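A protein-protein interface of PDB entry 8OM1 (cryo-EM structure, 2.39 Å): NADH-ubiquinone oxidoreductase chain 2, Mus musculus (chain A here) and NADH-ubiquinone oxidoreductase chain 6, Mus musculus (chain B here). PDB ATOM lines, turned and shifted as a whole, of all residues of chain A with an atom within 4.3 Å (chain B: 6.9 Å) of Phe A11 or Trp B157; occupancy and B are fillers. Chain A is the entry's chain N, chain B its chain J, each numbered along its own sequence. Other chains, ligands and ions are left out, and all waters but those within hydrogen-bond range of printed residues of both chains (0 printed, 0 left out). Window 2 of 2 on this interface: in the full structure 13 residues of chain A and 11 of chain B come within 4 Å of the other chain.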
ATOM      1  N   ALA A   7       2.812 -11.178 -21.521  1.00  0.00           N
ATOM      2  CA  ALA A   7       4.128 -10.653 -21.195  1.00  0.00           C
ATOM      3  C   ALA A   7       4.353 -10.629 -19.687  1.00  0.00           C
ATOM      4  O   ALA A   7       5.405 -11.054 -19.202  1.00  0.00           O
ATOM      5  CB  ALA A   7       4.280  -9.258 -21.789  1.00  0.00           C
ATOM      6  N   ILE A   8       3.373 -10.146 -18.931  1.00  0.00           N
ATOM      7  CA  ILE A   8       3.529 -10.048 -17.486  1.00  0.00           C
ATOM      8  C   ILE A   8       3.611 -11.438 -16.864  1.00  0.00           C
ATOM      9  O   ILE A   8       4.458 -11.700 -16.009  1.00  0.00           O
ATOM     10  CB  ILE A   8       2.383  -9.215 -16.881  1.00  0.00           C
ATOM     11  CG1 ILE A   8       2.711  -7.728 -16.972  1.00  0.00           C
ATOM     12  CG2 ILE A   8       2.130  -9.568 -15.425  1.00  0.00           C
ATOM     13  CD1 ILE A   8       1.521  -6.876 -17.177  1.00  0.00           C
ATOM     14  N   ILE A   9       2.730 -12.342 -17.276  1.00  0.00           N
ATOM     15  CA  ILE A   9       2.690 -13.657 -16.651  1.00  0.00           C
ATOM     16  C   ILE A   9       3.919 -14.471 -17.032  1.00  0.00           C
ATOM     17  O   ILE A   9       4.546 -15.098 -16.174  1.00  0.00           O
ATOM     18  CB  ILE A   9       1.378 -14.376 -17.005  1.00  0.00           C
ATOM     19  CG1 ILE A   9       0.217 -13.660 -16.305  1.00  0.00           C
ATOM     20  CG2 ILE A   9       1.452 -15.852 -16.600  1.00  0.00           C
ATOM     21  CD1 ILE A   9      -1.138 -14.237 -16.568  1.00  0.00           C
ATOM     22  N   TYR A  10       4.299 -14.463 -18.308  1.00  0.00           N
ATOM     23  CA  TYR A  10       5.491 -15.202 -18.710  1.00  0.00           C
ATOM     24  C   TYR A  10       6.745 -14.602 -18.101  1.00  0.00           C
ATOM     25  O   TYR A  10       7.681 -15.328 -17.762  1.00  0.00           O
ATOM     26  CB  TYR A  10       5.618 -15.249 -20.232  1.00  0.00           C
ATOM     27  CG  TYR A  10       4.938 -16.442 -20.844  1.00  0.00           C
ATOM     28  CD1 TYR A  10       5.418 -17.726 -20.626  1.00  0.00           C
ATOM     29  CD2 TYR A  10       3.814 -16.291 -21.634  1.00  0.00           C
ATOM     30  CE1 TYR A  10       4.793 -18.821 -21.180  1.00  0.00           C
ATOM     31  CE2 TYR A  10       3.183 -17.371 -22.189  1.00  0.00           C
ATOM     32  CZ  TYR A  10       3.674 -18.637 -21.966  1.00  0.00           C
ATOM     33  OH  TYR A  10       3.038 -19.720 -22.527  1.00  0.00           O
ATOM     34  N   PHE A  11       6.784 -13.278 -17.961  1.00  0.00           N
ATOM     35  CA  PHE A  11       7.919 -12.641 -17.311  1.00  0.00           C
ATOM     36  C   PHE A  11       8.033 -13.078 -15.855  1.00  0.00           C
ATOM     37  O   PHE A  11       9.135 -13.326 -15.359  1.00  0.00           O
ATOM     38  CB  PHE A  11       7.788 -11.125 -17.420  1.00  0.00           C
ATOM     39  CG  PHE A  11       8.848 -10.376 -16.685  1.00  0.00           C
ATOM     40  CD1 PHE A  11      10.125 -10.293 -17.189  1.00  0.00           C
ATOM     41  CD2 PHE A  11       8.570  -9.759 -15.486  1.00  0.00           C
ATOM     42  CE1 PHE A  11      11.100  -9.614 -16.516  1.00  0.00           C
ATOM     43  CE2 PHE A  11       9.544  -9.077 -14.808  1.00  0.00           C
ATOM     44  CZ  PHE A  11      10.812  -9.002 -15.323  1.00  0.00           C
ATOM     45  N   THR A  12       6.903 -13.178 -15.156  1.00  0.00           N
ATOM     46  CA  THR A  12       6.921 -13.636 -13.774  1.00  0.00           C
ATOM     47  C   THR A  12       7.283 -15.112 -13.668  1.00  0.00           C
ATOM     48  O   THR A  12       7.920 -15.516 -12.694  1.00  0.00           O
ATOM     49  CB  THR A  12       5.567 -13.365 -13.123  1.00  0.00           C
ATOM     50  OG1 THR A  12       5.143 -12.041 -13.454  1.00  0.00           O
ATOM     51  CG2 THR A  12       5.646 -13.514 -11.618  1.00  0.00           C
ATOM     52  N   ILE A  13       6.880 -15.926 -14.642  1.00  0.00           N
ATOM     53  CA  ILE A  13       7.289 -17.329 -14.659  1.00  0.00           C
ATOM     54  C   ILE A  13       8.802 -17.428 -14.805  1.00  0.00           C
ATOM     55  O   ILE A  13       9.455 -18.234 -14.138  1.00  0.00           O
ATOM     56  CB  ILE A  13       6.546 -18.089 -15.779  1.00  0.00           C
ATOM     57  CG1 ILE A  13       5.077 -18.284 -15.403  1.00  0.00           C
ATOM     58  CG2 ILE A  13       7.173 -19.443 -16.045  1.00  0.00           C
ATOM     59  CD1 ILE A  13       4.156 -18.515 -16.569  1.00  0.00           C
ATOM     60  N   PHE A  14       9.380 -16.603 -15.669  1.00  0.00           N
ATOM     61  CA  PHE A  14      10.825 -16.565 -15.833  1.00  0.00           C
ATOM     62  C   PHE A  14      11.514 -15.974 -14.608  1.00  0.00           C
ATOM     63  O   PHE A  14      12.588 -16.431 -14.210  1.00  0.00           O
ATOM     64  CB  PHE A  14      11.152 -15.762 -17.089  1.00  0.00           C
ATOM     65  CG  PHE A  14      12.602 -15.472 -17.274  1.00  0.00           C
ATOM     66  CD1 PHE A  14      13.462 -16.444 -17.753  1.00  0.00           C
ATOM     67  CD2 PHE A  14      13.109 -14.226 -16.986  1.00  0.00           C
ATOM     68  CE1 PHE A  14      14.790 -16.176 -17.932  1.00  0.00           C
ATOM     69  CE2 PHE A  14      14.440 -13.957 -17.166  1.00  0.00           C
ATOM     70  CZ  PHE A  14      15.279 -14.929 -17.640  1.00  0.00           C
ATOM     71  N   LEU A  15      10.905 -14.957 -14.000  1.00  0.00           N
ATOM     72  CA  LEU A  15      11.574 -14.181 -12.965  1.00  0.00           C
ATOM     73  C   LEU A  15      11.789 -14.990 -11.694  1.00  0.00           C
ATOM     74  O   LEU A  15      12.860 -14.911 -11.086  1.00  0.00           O
ATOM     75  CB  LEU A  15      10.759 -12.927 -12.660  1.00  0.00           C
ATOM     76  CG  LEU A  15      11.201 -12.028 -11.507  1.00  0.00           C
ATOM     77  CD1 LEU A  15      12.046 -10.879 -12.032  1.00  0.00           C
ATOM     78  CD2 LEU A  15       9.988 -11.534 -10.735  1.00  0.00           C
ATOM     79  N   PHE A  35       6.695 -16.600  -6.625  1.00  0.00           N
ATOM     80  CA  PHE A  35       6.373 -16.068  -7.945  1.00  0.00           C
ATOM     81  C   PHE A  35       6.041 -17.191  -8.914  1.00  0.00           C
ATOM     82  O   PHE A  35       5.124 -17.066  -9.729  1.00  0.00           O
ATOM     83  CB  PHE A  35       7.530 -15.231  -8.498  1.00  0.00           C
ATOM     84  CG  PHE A  35       7.543 -13.801  -8.031  1.00  0.00           C
ATOM     85  CD1 PHE A  35       6.411 -13.010  -8.099  1.00  0.00           C
ATOM     86  CD2 PHE A  35       8.699 -13.243  -7.534  1.00  0.00           C
ATOM     87  CE1 PHE A  35       6.440 -11.705  -7.670  1.00  0.00           C
ATOM     88  CE2 PHE A  35       8.727 -11.937  -7.108  1.00  0.00           C
ATOM     89  CZ  PHE A  35       7.597 -11.171  -7.175  1.00  0.00           C
ATOM     90  N   MET B 152      10.946  -4.242  -1.474  1.00  0.00           N
ATOM     91  CA  MET B 152       9.747  -3.557  -1.916  1.00  0.00           C
ATOM     92  C   MET B 152       9.505  -3.743  -3.406  1.00  0.00           C
ATOM     93  O   MET B 152       8.350  -3.764  -3.844  1.00  0.00           O
ATOM     94  CB  MET B 152       9.858  -2.080  -1.549  1.00  0.00           C
ATOM     95  CG  MET B 152       8.747  -1.208  -2.081  1.00  0.00           C
ATOM     96  SD  MET B 152       8.590   0.311  -1.130  1.00  0.00           S
ATOM     97  CE  MET B 152       7.783  -0.328   0.345  1.00  0.00           C
ATOM     98  N   VAL B 153      10.568  -3.889  -4.195  1.00  0.00           N
ATOM     99  CA  VAL B 153      10.404  -4.162  -5.619  1.00  0.00           C
ATOM    100  C   VAL B 153       9.679  -5.486  -5.823  1.00  0.00           C
ATOM    101  O   VAL B 153       8.726  -5.571  -6.603  1.00  0.00           O
ATOM    102  CB  VAL B 153      11.769  -4.139  -6.333  1.00  0.00           C
ATOM    103  CG1 VAL B 153      11.648  -4.687  -7.741  1.00  0.00           C
ATOM    104  CG2 VAL B 153      12.312  -2.733  -6.370  1.00  0.00           C
ATOM    105  N   VAL B 154      10.100  -6.534  -5.109  1.00  0.00           N
ATOM    106  CA  VAL B 154       9.480  -7.843  -5.299  1.00  0.00           C
ATOM    107  C   VAL B 154       8.064  -7.852  -4.740  1.00  0.00           C
ATOM    108  O   VAL B 154       7.169  -8.489  -5.300  1.00  0.00           O
ATOM    109  CB  VAL B 154      10.337  -8.973  -4.685  1.00  0.00           C
ATOM    110  CG1 VAL B 154      11.717  -9.001  -5.298  1.00  0.00           C
ATOM    111  CG2 VAL B 154      10.416  -8.866  -3.166  1.00  0.00           C
ATOM    112  N   ALA B 155       7.846  -7.186  -3.605  1.00  0.00           N
ATOM    113  CA  ALA B 155       6.506  -7.112  -3.038  1.00  0.00           C
ATOM    114  C   ALA B 155       5.563  -6.371  -3.971  1.00  0.00           C
ATOM    115  O   ALA B 155       4.430  -6.806  -4.198  1.00  0.00           O
ATOM    116  CB  ALA B 155       6.551  -6.430  -1.674  1.00  0.00           C
ATOM    117  N   GLY B 156       6.019  -5.247  -4.518  1.00  0.00           N
ATOM    118  CA  GLY B 156       5.197  -4.495  -5.439  1.00  0.00           C
ATOM    119  C   GLY B 156       4.906  -5.254  -6.716  1.00  0.00           C
ATOM    120  O   GLY B 156       3.798  -5.189  -7.246  1.00  0.00           O
ATOM    121  N   TRP B 157       5.898  -5.984  -7.231  1.00  0.00           N
ATOM    122  CA  TRP B 157       5.669  -6.750  -8.448  1.00  0.00           C
ATOM    123  C   TRP B 157       4.633  -7.842  -8.228  1.00  0.00           C
ATOM    124  O   TRP B 157       3.787  -8.085  -9.094  1.00  0.00           O
ATOM    125  CB  TRP B 157       6.966  -7.357  -8.975  1.00  0.00           C
ATOM    126  CG  TRP B 157       6.724  -8.010 -10.291  1.00  0.00           C
ATOM    127  CD1 TRP B 157       6.612  -9.339 -10.538  1.00  0.00           C
ATOM    128  CD2 TRP B 157       6.500  -7.350 -11.536  1.00  0.00           C
ATOM    129  NE1 TRP B 157       6.345  -9.551 -11.855  1.00  0.00           N
ATOM    130  CE2 TRP B 157       6.271  -8.344 -12.494  1.00  0.00           C
ATOM    131  CE3 TRP B 157       6.474  -6.011 -11.932  1.00  0.00           C
ATOM    132  CZ2 TRP B 157       6.030  -8.048 -13.833  1.00  0.00           C
ATOM    133  CZ3 TRP B 157       6.233  -5.718 -13.256  1.00  0.00           C
ATOM    134  CH2 TRP B 157       6.014  -6.733 -14.192  1.00  0.00           C
ATOM    135  N   SER B 158       4.680  -8.516  -7.081  1.00  0.00           N
ATOM    136  CA  SER B 158       3.749  -9.617  -6.849  1.00  0.00           C
ATOM    137  C   SER B 158       2.309  -9.122  -6.752  1.00  0.00           C
ATOM    138  O   SER B 158       1.394  -9.779  -7.252  1.00  0.00           O
ATOM    139  CB  SER B 158       4.156 -10.406  -5.604  1.00  0.00           C
ATOM    140  OG  SER B 158       3.631  -9.853  -4.422  1.00  0.00           O
ATOM    141  N   LEU B 159       2.082  -7.969  -6.126  1.00  0.00           N
ATOM    142  CA  LEU B 159       0.733  -7.411  -6.104  1.00  0.00           C
ATOM    143  C   LEU B 159       0.287  -6.975  -7.493  1.00  0.00           C
ATOM    144  O   LEU B 159      -0.872  -7.176  -7.867  1.00  0.00           O
ATOM    145  CB  LEU B 159       0.663  -6.244  -5.126  1.00  0.00           C
ATOM    146  CG  LEU B 159       0.831  -6.651  -3.660  1.00  0.00           C
ATOM    147  CD1 LEU B 159       1.090  -5.441  -2.773  1.00  0.00           C
ATOM    148  CD2 LEU B 159      -0.376  -7.447  -3.176  1.00  0.00           C
ATOM    149  N   PHE B 160       1.191  -6.377  -8.264  1.00  0.00           N
ATOM    150  CA  PHE B 160       0.866  -5.944  -9.618  1.00  0.00           C
ATOM    151  C   PHE B 160       0.562  -7.133 -10.520  1.00  0.00           C
ATOM    152  O   PHE B 160      -0.435  -7.135 -11.244  1.00  0.00           O
ATOM    153  CB  PHE B 160       2.026  -5.124 -10.171  1.00  0.00           C
ATOM    154  CG  PHE B 160       1.821  -4.638 -11.567  1.00  0.00           C
ATOM    155  CD1 PHE B 160       0.899  -3.638 -11.840  1.00  0.00           C
ATOM    156  CD2 PHE B 160       2.571  -5.154 -12.607  1.00  0.00           C
ATOM    157  CE1 PHE B 160       0.721  -3.182 -13.125  1.00  0.00           C
ATOM    158  CE2 PHE B 160       2.394  -4.699 -13.892  1.00  0.00           C
ATOM    159  CZ  PHE B 160       1.470  -3.709 -14.152  1.00  0.00           C
ATOM    160  N   ALA B 161       1.416  -8.154 -10.489  1.00  0.00           N
ATOM    161  CA  ALA B 161       1.166  -9.345 -11.283  1.00  0.00           C
ATOM    162  C   ALA B 161      -0.067 -10.086 -10.792  1.00  0.00           C
ATOM    163  O   ALA B 161      -0.773 -10.706 -11.592  1.00  0.00           O
ATOM    164  CB  ALA B 161       2.391 -10.261 -11.260  1.00  0.00           C
ATOM    165  N   GLY B 162      -0.350 -10.012  -9.491  1.00  0.00           N
ATOM    166  CA  GLY B 162      -1.536 -10.651  -8.954  1.00  0.00           C
ATOM    167  C   GLY B 162      -2.821 -10.157  -9.587  1.00  0.00           C
ATOM    168  O   GLY B 162      -3.763 -10.928  -9.766  1.00  0.00           O
ATOM    169  N   ILE B 163      -2.881  -8.874  -9.938  1.00  0.00           N
ATOM    170  CA  ILE B 163      -4.060  -8.347 -10.611  1.00  0.00           C
ATOM    171  C   ILE B 163      -4.255  -9.035 -11.958  1.00  0.00           C
ATOM    172  O   ILE B 163      -5.358  -9.472 -12.296  1.00  0.00           O
ATOM    173  CB  ILE B 163      -3.950  -6.822 -10.773  1.00  0.00           C
ATOM    174  CG1 ILE B 163      -4.023  -6.136  -9.408  1.00  0.00           C
ATOM    175  CG2 ILE B 163      -5.041  -6.314 -11.689  1.00  0.00           C
ATOM    176  CD1 ILE B 163      -3.506  -4.728  -9.415  1.00  0.00           C
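Printed residues of chain B that touch a printed residue of chain A: Val B154, Trp B157, Ser B158 and Ala B161. Hydrophobic or aromatic side chains of chain B within 4 Å of the printed part of chain A: Trp B157 and Ala B161. Hydrophobic or aromatic side chains of chain A that line the printed part of chain B: Phe A11 and Phe A35.
The indole nitrogen (NE1) of Trp B157 sits at hydrogen-bond distance from the side-chain hydroxyl (OG1) of Thr A12.
Phe A11 touches just one residue of chain B: Trp B157 (3.5 Å). Of chain A, only Phe A11 (3.5 Å), Thr A12 (3.2 Å) and Phe A35 (3.7 Å) come within 4 Å of Trp B157. Of the printed residues of chain A, Ala B161 touches Thr A12. Of the printed residues of chain B, Phe A35 touches Val B154, Trp B157 and Ser B158. Of the printed residues of chain A, Ser B158 touches Phe A35. Of the printed residues of chain A, Val B154 touches Phe A35. Ile B163 touches none of the printed residues of chain A. The nearest printed residue of chain B that does not touch Phe A11 is Ala B161 (7.5 Å). The nearest residue of chain A that does not touch Trp B157 is Leu A15 (4.03 Å). The nearest printed residue of chain A that does not touch Ser B158 is Thr A12 (6.4 Å).
CZ2 of Trp B157 touches CD2 of Phe A11 (3.5 Å). Ala B161 touches Thr A12. Phe A35 touches Val B154. CD1 of Trp B157 touches CE1 of Phe A35, at 3.7 Å. Phe A35 touches Ser B158 (CE1 to CB, 3.3 Å).
OG of Ser B158 is in hydrogen-bond range of O of Ala B155, at 3.2 Å. OG1 of Thr A12 is in hydrogen-bond range of O of Ile A8.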
